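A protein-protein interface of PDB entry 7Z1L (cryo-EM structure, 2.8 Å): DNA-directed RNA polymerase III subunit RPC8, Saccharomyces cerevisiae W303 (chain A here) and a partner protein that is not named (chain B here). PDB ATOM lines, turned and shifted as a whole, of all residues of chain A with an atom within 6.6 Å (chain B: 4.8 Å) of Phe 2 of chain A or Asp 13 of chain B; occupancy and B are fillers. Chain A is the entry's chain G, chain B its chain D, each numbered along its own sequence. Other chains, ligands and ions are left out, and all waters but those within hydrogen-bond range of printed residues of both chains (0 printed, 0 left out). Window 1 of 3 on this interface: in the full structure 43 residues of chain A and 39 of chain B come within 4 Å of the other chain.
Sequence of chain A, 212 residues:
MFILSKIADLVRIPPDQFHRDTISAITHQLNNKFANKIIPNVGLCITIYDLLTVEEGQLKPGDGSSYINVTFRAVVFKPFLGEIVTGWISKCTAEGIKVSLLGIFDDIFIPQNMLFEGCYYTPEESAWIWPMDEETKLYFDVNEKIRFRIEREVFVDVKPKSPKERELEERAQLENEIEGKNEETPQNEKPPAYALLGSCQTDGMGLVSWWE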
ATOM      1  N   MET A   1     -16.029   2.944   1.207  1.00  0.00           N
ATOM      2  CA  MET A   1     -17.417   3.327   1.431  1.00  0.00           C
ATOM      3  C   MET A   1     -17.548   4.115   2.730  1.00  0.00           C
ATOM      4  O   MET A   1     -18.239   5.132   2.785  1.00  0.00           O
ATOM      5  CB  MET A   1     -18.314   2.091   1.460  1.00  0.00           C
ATOM      6  CG  MET A   1     -19.791   2.396   1.607  1.00  0.00           C
ATOM      7  SD  MET A   1     -20.791   0.899   1.539  1.00  0.00           S
ATOM      8  CE  MET A   1     -22.421   1.569   1.841  1.00  0.00           C
ATOM      9  N   PHE A   2     -16.878   3.636   3.774  1.00  0.00           N
ATOM     10  CA  PHE A   2     -16.791   4.330   5.050  1.00  0.00           C
ATOM     11  C   PHE A   2     -15.332   4.655   5.323  1.00  0.00           C
ATOM     12  O   PHE A   2     -14.472   3.775   5.222  1.00  0.00           O
ATOM     13  CB  PHE A   2     -17.359   3.479   6.189  1.00  0.00           C
ATOM     14  CG  PHE A   2     -18.823   3.180   6.057  1.00  0.00           C
ATOM     15  CD1 PHE A   2     -19.749   4.203   5.972  1.00  0.00           C
ATOM     16  CD2 PHE A   2     -19.273   1.871   6.026  1.00  0.00           C
ATOM     17  CE1 PHE A   2     -21.097   3.927   5.853  1.00  0.00           C
ATOM     18  CE2 PHE A   2     -20.619   1.591   5.907  1.00  0.00           C
ATOM     19  CZ  PHE A   2     -21.531   2.619   5.820  1.00  0.00           C
ATOM     20  N   ILE A   3     -15.050   5.913   5.667  1.00  0.00           N
ATOM     21  CA  ILE A   3     -13.693   6.345   5.980  1.00  0.00           C
ATOM     22  C   ILE A   3     -13.712   7.120   7.291  1.00  0.00           C
ATOM     23  O   ILE A   3     -14.765   7.381   7.874  1.00  0.00           O
ATOM     24  CB  ILE A   3     -13.065   7.198   4.855  1.00  0.00           C
ATOM     25  CG1 ILE A   3     -13.992   8.344   4.462  1.00  0.00           C
ATOM     26  CG2 ILE A   3     -12.749   6.339   3.647  1.00  0.00           C
ATOM     27  CD1 ILE A   3     -13.428   9.243   3.385  1.00  0.00           C
ATOM     28  N   LEU A   4     -12.519   7.468   7.762  1.00  0.00           N
ATOM     29  CA  LEU A   4     -12.339   8.209   9.003  1.00  0.00           C
ATOM     30  C   LEU A   4     -11.890   9.627   8.686  1.00  0.00           C
ATOM     31  O   LEU A   4     -10.943   9.824   7.919  1.00  0.00           O
ATOM     32  CB  LEU A   4     -11.315   7.524   9.908  1.00  0.00           C
ATOM     33  CG  LEU A   4     -11.780   6.283  10.665  1.00  0.00           C
ATOM     34  CD1 LEU A   4     -10.690   5.803  11.603  1.00  0.00           C
ATOM     35  CD2 LEU A   4     -13.050   6.586  11.434  1.00  0.00           C
ATOM     36  N   LEU A  44     -21.275  12.278   4.473  1.00  0.00           N
ATOM     37  CA  LEU A  44     -22.310  12.106   5.486  1.00  0.00           C
ATOM     38  C   LEU A  44     -21.708  11.398   6.692  1.00  0.00           C
ATOM     39  O   LEU A  44     -21.178  10.290   6.562  1.00  0.00           O
ATOM     40  CB  LEU A  44     -23.492  11.313   4.928  1.00  0.00           C
ATOM     41  CG  LEU A  44     -24.662  10.999   5.862  1.00  0.00           C
ATOM     42  CD1 LEU A  44     -25.981  11.274   5.164  1.00  0.00           C
ATOM     43  CD2 LEU A  44     -24.610   9.554   6.326  1.00  0.00           C
ATOM     44  N   ILE A  46     -21.753   9.450  10.308  1.00  0.00           N
ATOM     45  CA  ILE A  46     -22.612   8.497  11.000  1.00  0.00           C
ATOM     46  C   ILE A  46     -22.409   8.631  12.502  1.00  0.00           C
ATOM     47  O   ILE A  46     -23.335   8.994  13.236  1.00  0.00           O
ATOM     48  CB  ILE A  46     -22.336   7.052  10.544  1.00  0.00           C
ATOM     49  CG1 ILE A  46     -22.634   6.887   9.055  1.00  0.00           C
ATOM     50  CG2 ILE A  46     -23.161   6.068  11.355  1.00  0.00           C
ATOM     51  CD1 ILE A  46     -21.395   6.866   8.198  1.00  0.00           C
ATOM     52  N   VAL A  75     -16.599   8.494  11.693  1.00  0.00           N
ATOM     53  CA  VAL A  75     -16.895   7.610  10.571  1.00  0.00           C
ATOM     54  C   VAL A  75     -17.809   8.365   9.613  1.00  0.00           C
ATOM     55  O   VAL A  75     -18.931   8.730   9.971  1.00  0.00           O
ATOM     56  CB  VAL A  75     -17.551   6.310  11.046  1.00  0.00           C
ATOM     57  CG1 VAL A  75     -17.815   5.383   9.871  1.00  0.00           C
ATOM     58  CG2 VAL A  75     -16.698   5.636  12.108  1.00  0.00           C
ATOM     59  N   VAL A  76     -17.338   8.594   8.392  1.00  0.00           N
ATOM     60  CA  VAL A  76     -18.089   9.325   7.381  1.00  0.00           C
ATOM     61  C   VAL A  76     -18.287   8.429   6.163  1.00  0.00           C
ATOM     62  O   VAL A  76     -17.365   7.726   5.729  1.00  0.00           O
ATOM     63  CB  VAL A  76     -17.394  10.658   7.023  1.00  0.00           C
ATOM     64  CG1 VAL A  76     -15.969  10.434   6.584  1.00  0.00           C
ATOM     65  CG2 VAL A  76     -18.167  11.408   5.949  1.00  0.00           C
ATOM     66  N   PHE A  77     -19.514   8.428   5.643  1.00  0.00           N
ATOM     67  CA  PHE A  77     -19.902   7.604   4.501  1.00  0.00           C
ATOM     68  C   PHE A  77     -19.563   8.376   3.232  1.00  0.00           C
ATOM     69  O   PHE A  77     -20.266   9.315   2.852  1.00  0.00           O
ATOM     70  CB  PHE A  77     -21.385   7.257   4.586  1.00  0.00           C
ATOM     71  CG  PHE A  77     -21.988   6.792   3.293  1.00  0.00           C
ATOM     72  CD1 PHE A  77     -21.705   5.533   2.795  1.00  0.00           C
ATOM     73  CD2 PHE A  77     -22.868   7.600   2.595  1.00  0.00           C
ATOM     74  CE1 PHE A  77     -22.270   5.100   1.612  1.00  0.00           C
ATOM     75  CE2 PHE A  77     -23.433   7.171   1.413  1.00  0.00           C
ATOM     76  CZ  PHE A  77     -23.135   5.920   0.922  1.00  0.00           C
ATOM     77  N   LYS A  78     -18.466   7.993   2.584  1.00  0.00           N
ATOM     78  CA  LYS A  78     -17.996   8.651   1.365  1.00  0.00           C
ATOM     79  C   LYS A  78     -17.490   7.597   0.395  1.00  0.00           C
ATOM     80  O   LYS A  78     -16.316   7.211   0.427  1.00  0.00           O
ATOM     81  CB  LYS A  78     -16.902   9.674   1.676  1.00  0.00           C
ATOM     82  CG  LYS A  78     -16.543  10.561   0.500  1.00  0.00           C
ATOM     83  CD  LYS A  78     -15.151  11.144   0.653  1.00  0.00           C
ATOM     84  CE  LYS A  78     -14.899  12.232  -0.373  1.00  0.00           C
ATOM     85  NZ  LYS A  78     -13.471  12.649  -0.390  1.00  0.00           N
ATOM     86  N   PRO A  79     -18.362   7.090  -0.477  1.00  0.00           N
ATOM     87  CA  PRO A  79     -17.912   6.141  -1.506  1.00  0.00           C
ATOM     88  C   PRO A  79     -16.954   6.808  -2.480  1.00  0.00           C
ATOM     89  O   PRO A  79     -17.287   7.806  -3.124  1.00  0.00           O
ATOM     90  CB  PRO A  79     -19.216   5.720  -2.193  1.00  0.00           C
ATOM     91  CG  PRO A  79     -20.285   6.022  -1.207  1.00  0.00           C
ATOM     92  CD  PRO A  79     -19.825   7.237  -0.465  1.00  0.00           C
ATOM     93  N   GLU A  83     -15.990   2.928  -6.878  1.00  0.00           N
ATOM     94  CA  GLU A  83     -16.531   1.869  -6.037  1.00  0.00           C
ATOM     95  C   GLU A  83     -17.961   1.538  -6.449  1.00  0.00           C
ATOM     96  O   GLU A  83     -18.756   2.428  -6.759  1.00  0.00           O
ATOM     97  CB  GLU A  83     -16.495   2.289  -4.569  1.00  0.00           C
ATOM     98  CG  GLU A  83     -16.788   1.161  -3.591  1.00  0.00           C
ATOM     99  CD  GLU A  83     -16.868   1.641  -2.157  1.00  0.00           C
ATOM    100  OE1 GLU A  83     -16.963   2.868  -1.942  1.00  0.00           O
ATOM    101  OE2 GLU A  83     -16.836   0.790  -1.243  1.00  0.00           O
ATOM    102  N   ILE A 104     -30.362   4.856   4.587  1.00  0.00           N
ATOM    103  CA  ILE A 104     -29.200   5.621   5.037  1.00  0.00           C
ATOM    104  C   ILE A 104     -29.010   6.871   4.181  1.00  0.00           C
ATOM    105  O   ILE A 104     -28.640   7.935   4.690  1.00  0.00           O
ATOM    106  CB  ILE A 104     -27.934   4.740   5.060  1.00  0.00           C
ATOM    107  CG1 ILE A 104     -26.729   5.531   5.572  1.00  0.00           C
ATOM    108  CG2 ILE A 104     -27.615   4.167   3.702  1.00  0.00           C
ATOM    109  CD1 ILE A 104     -25.469   4.710   5.677  1.00  0.00           C
ATOM    110  N   PHE B  10      -9.039   4.072   6.137  1.00  0.00           N
ATOM    111  CA  PHE B  10     -10.068   3.331   5.426  1.00  0.00           C
ATOM    112  C   PHE B  10     -10.697   2.321   6.372  1.00  0.00           C
ATOM    113  O   PHE B  10      -9.988   1.541   7.015  1.00  0.00           O
ATOM    114  CB  PHE B  10      -9.486   2.619   4.205  1.00  0.00           C
ATOM    115  CG  PHE B  10      -9.658   3.378   2.928  1.00  0.00           C
ATOM    116  CD1 PHE B  10     -10.915   3.555   2.382  1.00  0.00           C
ATOM    117  CD2 PHE B  10      -8.564   3.916   2.272  1.00  0.00           C
ATOM    118  CE1 PHE B  10     -11.084   4.251   1.206  1.00  0.00           C
ATOM    119  CE2 PHE B  10      -8.726   4.615   1.094  1.00  0.00           C
ATOM    120  CZ  PHE B  10      -9.989   4.783   0.563  1.00  0.00           C
ATOM    121  N   LEU B  11     -12.022   2.339   6.455  1.00  0.00           N
ATOM    122  CA  LEU B  11     -12.763   1.432   7.319  1.00  0.00           C
ATOM    123  C   LEU B  11     -13.434   0.365   6.468  1.00  0.00           C
ATOM    124  O   LEU B  11     -14.188   0.685   5.542  1.00  0.00           O
ATOM    125  CB  LEU B  11     -13.807   2.186   8.140  1.00  0.00           C
ATOM    126  CG  LEU B  11     -13.322   3.051   9.300  1.00  0.00           C
ATOM    127  CD1 LEU B  11     -14.503   3.431  10.165  1.00  0.00           C
ATOM    128  CD2 LEU B  11     -12.267   2.328  10.118  1.00  0.00           C
ATOM    129  N   SER B  12     -13.160  -0.897   6.780  1.00  0.00           N
ATOM    130  CA  SER B  12     -13.911  -1.984   6.179  1.00  0.00           C
ATOM    131  C   SER B  12     -15.321  -2.013   6.753  1.00  0.00           C
ATOM    132  O   SER B  12     -15.581  -1.491   7.841  1.00  0.00           O
ATOM    133  CB  SER B  12     -13.214  -3.321   6.428  1.00  0.00           C
ATOM    134  OG  SER B  12     -13.436  -3.768   7.753  1.00  0.00           O
ATOM    135  N   ASP B  13     -16.242  -2.620   6.002  1.00  0.00           N
ATOM    136  CA  ASP B  13     -17.612  -2.745   6.490  1.00  0.00           C
ATOM    137  C   ASP B  13     -17.687  -3.637   7.721  1.00  0.00           C
ATOM    138  O   ASP B  13     -18.583  -3.465   8.556  1.00  0.00           O
ATOM    139  CB  ASP B  13     -18.521  -3.277   5.384  1.00  0.00           C
ATOM    140  CG  ASP B  13     -18.809  -2.238   4.319  1.00  0.00           C
ATOM    141  OD1 ASP B  13     -18.217  -1.142   4.384  1.00  0.00           O
ATOM    142  OD2 ASP B  13     -19.627  -2.518   3.418  1.00  0.00           O
ATOM    143  N   TYR B  14     -16.757  -4.588   7.856  1.00  0.00           N
ATOM    144  CA  TYR B  14     -16.709  -5.406   9.063  1.00  0.00           C
ATOM    145  C   TYR B  14     -16.372  -4.565  10.287  1.00  0.00           C
ATOM    146  O   TYR B  14     -16.971  -4.746  11.352  1.00  0.00           O
ATOM    147  CB  TYR B  14     -15.690  -6.533   8.908  1.00  0.00           C
ATOM    148  CG  TYR B  14     -15.334  -7.193  10.221  1.00  0.00           C
ATOM    149  CD1 TYR B  14     -16.271  -7.944  10.918  1.00  0.00           C
ATOM    150  CD2 TYR B  14     -14.069  -7.048  10.774  1.00  0.00           C
ATOM    151  CE1 TYR B  14     -15.954  -8.543  12.120  1.00  0.00           C
ATOM    152  CE2 TYR B  14     -13.742  -7.645  11.977  1.00  0.00           C
ATOM    153  CZ  TYR B  14     -14.689  -8.390  12.644  1.00  0.00           C
ATOM    154  OH  TYR B  14     -14.370  -8.985  13.843  1.00  0.00           O
ATOM    155  N   GLU B  15     -15.406  -3.650  10.158  1.00  0.00           N
ATOM    156  CA  GLU B  15     -15.041  -2.790  11.280  1.00  0.00           C
ATOM    157  C   GLU B  15     -16.200  -1.892  11.688  1.00  0.00           C
ATOM    158  O   GLU B  15     -16.482  -1.734  12.882  1.00  0.00           O
ATOM    159  CB  GLU B  15     -13.818  -1.946  10.924  1.00  0.00           C
ATOM    160  CG  GLU B  15     -12.533  -2.737  10.766  1.00  0.00           C
ATOM    161  CD  GLU B  15     -11.326  -1.845  10.550  1.00  0.00           C
ATOM    162  OE1 GLU B  15     -11.244  -0.785  11.205  1.00  0.00           O
ATOM    163  OE2 GLU B  15     -10.462  -2.203   9.723  1.00  0.00           O
ATOM    164  N   VAL B  16     -16.890  -1.307  10.705  1.00  0.00           N
ATOM    165  CA  VAL B  16     -18.033  -0.445  10.992  1.00  0.00           C
ATOM    166  C   VAL B  16     -19.146  -1.242  11.659  1.00  0.00           C
ATOM    167  O   VAL B  16     -19.741  -0.796  12.650  1.00  0.00           O
ATOM    168  CB  VAL B  16     -18.515   0.238   9.697  1.00  0.00           C
ATOM    169  CG1 VAL B  16     -19.930   0.775   9.856  1.00  0.00           C
ATOM    170  CG2 VAL B  16     -17.560   1.351   9.304  1.00  0.00           C
ATOM    171  N   LEU B  17     -19.431  -2.440  11.141  1.00  0.00           N
ATOM    172  CA  LEU B  17     -20.483  -3.275  11.712  1.00  0.00           C
ATOM    173  C   LEU B  17     -20.150  -3.686  13.142  1.00  0.00           C
ATOM    174  O   LEU B  17     -21.008  -3.634  14.029  1.00  0.00           O
ATOM    175  CB  LEU B  17     -20.702  -4.505  10.833  1.00  0.00           C
ATOM    176  CG  LEU B  17     -21.845  -5.440  11.228  1.00  0.00           C
ATOM    177  CD1 LEU B  17     -23.130  -4.657  11.423  1.00  0.00           C
ATOM    178  CD2 LEU B  17     -22.031  -6.521  10.179  1.00  0.00           C
ATOM    179  N   VAL B  62     -27.699   1.605   9.457  1.00  0.00           N
ATOM    180  CA  VAL B  62     -26.431   1.030   9.014  1.00  0.00           C
ATOM    181  C   VAL B  62     -26.323  -0.434   9.431  1.00  0.00           C
ATOM    182  O   VAL B  62     -25.850  -1.275   8.658  1.00  0.00           O
ATOM    183  CB  VAL B  62     -25.239   1.856   9.532  1.00  0.00           C
ATOM    184  CG1 VAL B  62     -23.929   1.208   9.119  1.00  0.00           C
ATOM    185  CG2 VAL B  62     -25.293   3.261   8.987  1.00  0.00           C
ATOM    186  N   LEU B  66     -25.918  -3.484   6.790  1.00  0.00           N
ATOM    187  CA  LEU B  66     -24.785  -4.397   6.846  1.00  0.00           C
ATOM    188  C   LEU B  66     -25.156  -5.770   7.390  1.00  0.00           C
ATOM    189  O   LEU B  66     -24.368  -6.710   7.243  1.00  0.00           O
ATOM    190  CB  LEU B  66     -23.666  -3.794   7.700  1.00  0.00           C
ATOM    191  CG  LEU B  66     -23.030  -2.494   7.201  1.00  0.00           C
ATOM    192  CD1 LEU B  66     -21.915  -2.053   8.134  1.00  0.00           C
ATOM    193  CD2 LEU B  66     -22.503  -2.663   5.788  1.00  0.00           C
ATOM    194  N   LYS B  70     -25.231  -9.563   1.672  1.00  0.00           N
ATOM    195  CA  LYS B  70     -24.619  -8.903   0.530  1.00  0.00           C
ATOM    196  C   LYS B  70     -25.160  -9.517  -0.751  1.00  0.00           C
ATOM    197  O   LYS B  70     -25.365 -10.731  -0.833  1.00  0.00           O
ATOM    198  CB  LYS B  70     -23.096  -9.033   0.590  1.00  0.00           C
ATOM    199  CG  LYS B  70     -22.398  -8.421   1.820  1.00  0.00           C
ATOM    200  CD  LYS B  70     -22.394  -6.883   1.845  1.00  0.00           C
ATOM    201  CE  LYS B  70     -23.556  -6.276   2.630  1.00  0.00           C
ATOM    202  NZ  LYS B  70     -23.452  -4.792   2.716  1.00  0.00           N
ATOM    203  N   ILE B  95     -20.129 -10.764   6.817  1.00  0.00           N
ATOM    204  CA  ILE B  95     -19.328  -9.868   7.648  1.00  0.00           C
ATOM    205  C   ILE B  95     -19.858  -9.841   9.074  1.00  0.00           C
ATOM    206  O   ILE B  95     -19.102  -9.593  10.021  1.00  0.00           O
ATOM    207  CB  ILE B  95     -19.278  -8.456   7.029  1.00  0.00           C
ATOM    208  CG1 ILE B  95     -20.688  -7.891   6.847  1.00  0.00           C
ATOM    209  CG2 ILE B  95     -18.531  -8.482   5.705  1.00  0.00           C
ATOM    210  CD1 ILE B  95     -20.730  -6.564   6.121  1.00  0.00           C
ATOM    211  N   ASN B 125     -15.427  -5.710   1.588  1.00  0.00           N
ATOM    212  CA  ASN B 125     -16.745  -5.152   1.878  1.00  0.00           C
ATOM    213  C   ASN B 125     -17.860  -6.038   1.337  1.00  0.00           C
ATOM    214  O   ASN B 125     -18.821  -6.347   2.051  1.00  0.00           O
ATOM    215  CB  ASN B 125     -16.867  -3.740   1.306  1.00  0.00           C
ATOM    216  CG  ASN B 125     -16.010  -2.736   2.042  1.00  0.00           C
ATOM    217  OD1 ASN B 125     -15.926  -2.754   3.269  1.00  0.00           O
ATOM    218  ND2 ASN B 125     -15.380  -1.841   1.295  1.00  0.00           N
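N of Leu 11 of chain B lies within hydrogen-bond range of O of Phe 2 of chain A, at 3.1 Å.
Of the 13 printed residues of chain B, 6 touch a printed residue of chain A.
Hydrophobic or aromatic side chains of chain B that line the printed part of chain A: Phe 10, Leu 11, Val 16 and Val 62.
Of the 13 printed residues of chain A, 6 touch a printed residue of chain B.
Printed residues of chain A that touch a printed residue of chain B: Phe 2, Ile 3, Leu 4, Val 75, Glu 83 and Ile 104.
Among the printed residues, no Asp or Glu carboxylate lies within 4 Å of a Lys or Arg side-chain nitrogen of the other chain.
Phe 2 of chain A touches three residues of chain B.
Printed residues of chain B within 4 Å of Leu 4 of chain A: Leu 11.
Of the printed residues of chain B, Val 75 of chain A touches Leu 11.
Of the printed residues of chain B, Ile 104 of chain A touches Val 62.
Of the printed residues of chain A, Leu 11 of chain B touches Phe 2, Leu 4 and Val 75.
Printed residues of chain A within 4 Å of Val 16 of chain B: Phe 2 (3.7 Å).
The nearest residue of chain B that does not touch Phe 2 of chain A is Phe 10 of chain B (4.2 Å).
The nearest printed residue of chain B that does not touch Ile 104 of chain A is Leu 66 of chain B (7.8 Å).
The backbone NH of Val 76 of chain A sits at hydrogen-bond distance from the backbone carbonyl oxygen of Ile 3 of chain A, 2.9 Å away.
The backbone carbonyl oxygen (O) of Val 75 of chain A sits at hydrogen-bond distance from the backbone NH (N) of Ile 46 of chain A.
The side-chain carboxylate (OE1) of Glu 83 of chain A is in hydrogen-bond range of the backbone NH (N) of Met 1 of chain A (3.3 Å).
The side-chain amide oxygen (OD1) of Asn 125 of chain B sits at hydrogen-bond distance from the backbone NH (N) of Asp 13 of chain B, at 2.8 Å.
Among the printed residues, merely in contact across the chains: Phe 2 of chain A with Asp 13 of chain B (3.6 Å), Phe 2 of chain A with Val 16 of chain B (3.7 Å), Ile 3 of chain A with Phe 10 of chain B (3.6 Å), Leu 4 of chain A with Leu 11 of chain B (3.7 Å), Val 75 of chain A with Leu 11 of chain B (3.7 Å), Glu 83 of chain A with Asn 125 of chain B (3.9 Å) and Ile 104 of chain A with Val 62 of chain B (3.6 Å).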
